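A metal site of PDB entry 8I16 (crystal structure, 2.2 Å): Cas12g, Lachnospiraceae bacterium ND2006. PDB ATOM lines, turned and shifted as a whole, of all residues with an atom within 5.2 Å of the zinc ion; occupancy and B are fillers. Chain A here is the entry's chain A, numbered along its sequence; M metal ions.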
ATOM      1  N   HIS A 248       9.513 -13.494  -5.002  1.00  0.00           N
ATOM      2  CA  HIS A 248       8.386 -13.309  -5.969  1.00  0.00           C
ATOM      3  C   HIS A 248       7.334 -12.395  -5.338  1.00  0.00           C
ATOM      4  O   HIS A 248       7.338 -12.268  -4.124  1.00  0.00           O
ATOM      5  CB  HIS A 248       7.695 -14.626  -6.328  1.00  0.00           C
ATOM      6  CG  HIS A 248       8.497 -15.585  -7.137  1.00  0.00           C
ATOM      7  ND1 HIS A 248       8.363 -15.667  -8.513  1.00  0.00           N
ATOM      8  CD2 HIS A 248       9.346 -16.568  -6.771  1.00  0.00           C
ATOM      9  CE1 HIS A 248       9.138 -16.628  -8.962  1.00  0.00           C
ATOM     10  NE2 HIS A 248       9.756 -17.208  -7.916  1.00  0.00           N
ATOM     11  N   SER A 249       6.425 -11.850  -6.143  1.00  0.00           N
ATOM     12  CA  SER A 249       5.218 -11.118  -5.662  1.00  0.00           C
ATOM     13  C   SER A 249       4.321 -12.049  -4.827  1.00  0.00           C
ATOM     14  O   SER A 249       4.446 -13.310  -4.928  1.00  0.00           O
ATOM     15  CB  SER A 249       4.487 -10.462  -6.846  1.00  0.00           C
ATOM     16  OG  SER A 249       3.081 -10.460  -6.680  1.00  0.00           O
ATOM     17  N   CYS A 252       2.221 -14.334  -7.009  1.00  0.00           N
ATOM     18  CA  CYS A 252       2.973 -15.524  -7.509  1.00  0.00           C
ATOM     19  C   CYS A 252       2.909 -16.641  -6.472  1.00  0.00           C
ATOM     20  O   CYS A 252       2.878 -17.822  -6.885  1.00  0.00           O
ATOM     21  CB  CYS A 252       4.417 -15.193  -7.866  1.00  0.00           C
ATOM     22  SG  CYS A 252       4.624 -13.577  -8.677  1.00  0.00           S
ATOM     23  N   HIS A 322       1.457 -12.471 -12.608  1.00  0.00           N
ATOM     24  CA  HIS A 322       2.190 -13.299 -11.638  1.00  0.00           C
ATOM     25  C   HIS A 322       2.950 -14.354 -12.418  1.00  0.00           C
ATOM     26  O   HIS A 322       2.539 -14.648 -13.538  1.00  0.00           O
ATOM     27  CB  HIS A 322       1.239 -13.918 -10.602  1.00  0.00           C
ATOM     28  CG  HIS A 322       0.186 -14.802 -11.183  1.00  0.00           C
ATOM     29  ND1 HIS A 322       0.444 -16.104 -11.615  1.00  0.00           N
ATOM     30  CD2 HIS A 322      -1.137 -14.597 -11.375  1.00  0.00           C
ATOM     31  CE1 HIS A 322      -0.677 -16.654 -12.061  1.00  0.00           C
ATOM     32  NE2 HIS A 322      -1.661 -15.752 -11.927  1.00  0.00           N
ATOM     33  N   CYS A 323       4.020 -14.868 -11.818  1.00  0.00           N
ATOM     34  CA  CYS A 323       4.883 -15.928 -12.359  1.00  0.00           C
ATOM     35  C   CYS A 323       4.001 -17.193 -12.481  1.00  0.00           C
ATOM     36  O   CYS A 323       2.879 -17.217 -11.903  1.00  0.00           O
ATOM     37  CB  CYS A 323       6.135 -16.023 -11.484  1.00  0.00           C
ATOM     38  SG  CYS A 323       7.209 -14.548 -11.595  1.00  0.00           S
ATOM     39  N   ASN A 325       5.609 -20.397 -12.246  1.00  0.00           N
ATOM     40  CA  ASN A 325       6.406 -21.224 -11.295  1.00  0.00           C
ATOM     41  C   ASN A 325       6.919 -20.324 -10.162  1.00  0.00           C
ATOM     42  O   ASN A 325       6.934 -19.086 -10.350  1.00  0.00           O
ATOM     43  CB  ASN A 325       7.657 -21.843 -11.925  1.00  0.00           C
ATOM     44  CG  ASN A 325       7.349 -23.008 -12.839  1.00  0.00           C
ATOM     45  OD1 ASN A 325       7.003 -24.090 -12.376  1.00  0.00           O
ATOM     46  ND2 ASN A 325       7.500 -22.805 -14.138  1.00  0.00           N
ATOM     47  N   CYS A 330      11.206 -13.682 -10.662  1.00  0.00           N
ATOM     48  CA  CYS A 330       9.933 -13.008 -10.890  1.00  0.00           C
ATOM     49  C   CYS A 330      10.057 -11.662 -11.604  1.00  0.00           C
ATOM     50  O   CYS A 330      11.016 -10.919 -11.393  1.00  0.00           O
ATOM     51  CB  CYS A 330       9.172 -12.829  -9.571  1.00  0.00           C
ATOM     52  SG  CYS A 330       7.722 -11.766  -9.686  1.00  0.00           S
ATOM     53  N   GLU A 331       9.079 -11.366 -12.458  1.00  0.00           N
ATOM     54  CA  GLU A 331       9.028 -10.098 -13.223  1.00  0.00           C
ATOM     55  C   GLU A 331       7.830  -9.289 -12.726  1.00  0.00           C
ATOM     56  O   GLU A 331       7.510  -8.256 -13.358  1.00  0.00           O
ATOM     57  CB  GLU A 331       9.024 -10.355 -14.733  1.00  0.00           C
ATOM     58  CG  GLU A 331       8.203 -11.557 -15.204  1.00  0.00           C
ATOM     59  CD  GLU A 331       8.980 -12.820 -15.550  1.00  0.00           C
ATOM     60  OE1 GLU A 331       8.583 -13.514 -16.530  1.00  0.00           O
ATOM     61  OE2 GLU A 331       9.975 -13.132 -14.852  1.00  0.00           O
ATOM     62  N   PHE A 332       7.221  -9.681 -11.591  1.00  0.00           N
ATOM     63  CA  PHE A 332       6.018  -8.986 -11.050  1.00  0.00           C
ATOM     64  C   PHE A 332       6.331  -8.450  -9.661  1.00  0.00           C
ATOM     65  O   PHE A 332       5.399  -7.991  -8.963  1.00  0.00           O
ATOM     66  CB  PHE A 332       4.797  -9.913 -11.111  1.00  0.00           C
ATOM     67  CG  PHE A 332       4.565 -10.465 -12.496  1.00  0.00           C
ATOM     68  CD1 PHE A 332       3.945  -9.686 -13.466  1.00  0.00           C
ATOM     69  CD2 PHE A 332       5.072 -11.707 -12.860  1.00  0.00           C
ATOM     70  CE1 PHE A 332       3.793 -10.176 -14.757  1.00  0.00           C
ATOM     71  CE2 PHE A 332       4.915 -12.180 -14.152  1.00  0.00           C
ATOM     72  CZ  PHE A 332       4.273 -11.419 -15.102  1.00  0.00           C
HETATM   73 ZN    ZN M   1       6.908 -14.297  -9.353  1.00  0.00          ZN
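The side-chain sulfur of Cys 330 lies close to the backbone NH of Ser 249 (3.8 Å). The backbone NH (N) of Phe 332 lies close to the side-chain sulfur (SG) of Cys 330, at 2.9 Å. SG of Cys 323 lies close to N of Glu 331 (3.8 Å). The side-chain sulfur of Cys 252 lies close to the backbone NH of Ser 249 (3.6 Å).
The zinc ion is bound by a ring nitrogen (ND1) of His 248 (2.2 Å), the side-chain sulfur (SG) of Cys 323 (2.3 Å), the side-chain sulfur (SG) of Cys 252 (2.5 Å) and the side-chain sulfur (SG) of Cys 330 (2.7 Å). The zinc ion has four donor atoms within binding distance.
Within 4 Å of the zinc ion: His 248, Cys 252, Cys 323 and Cys 330.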
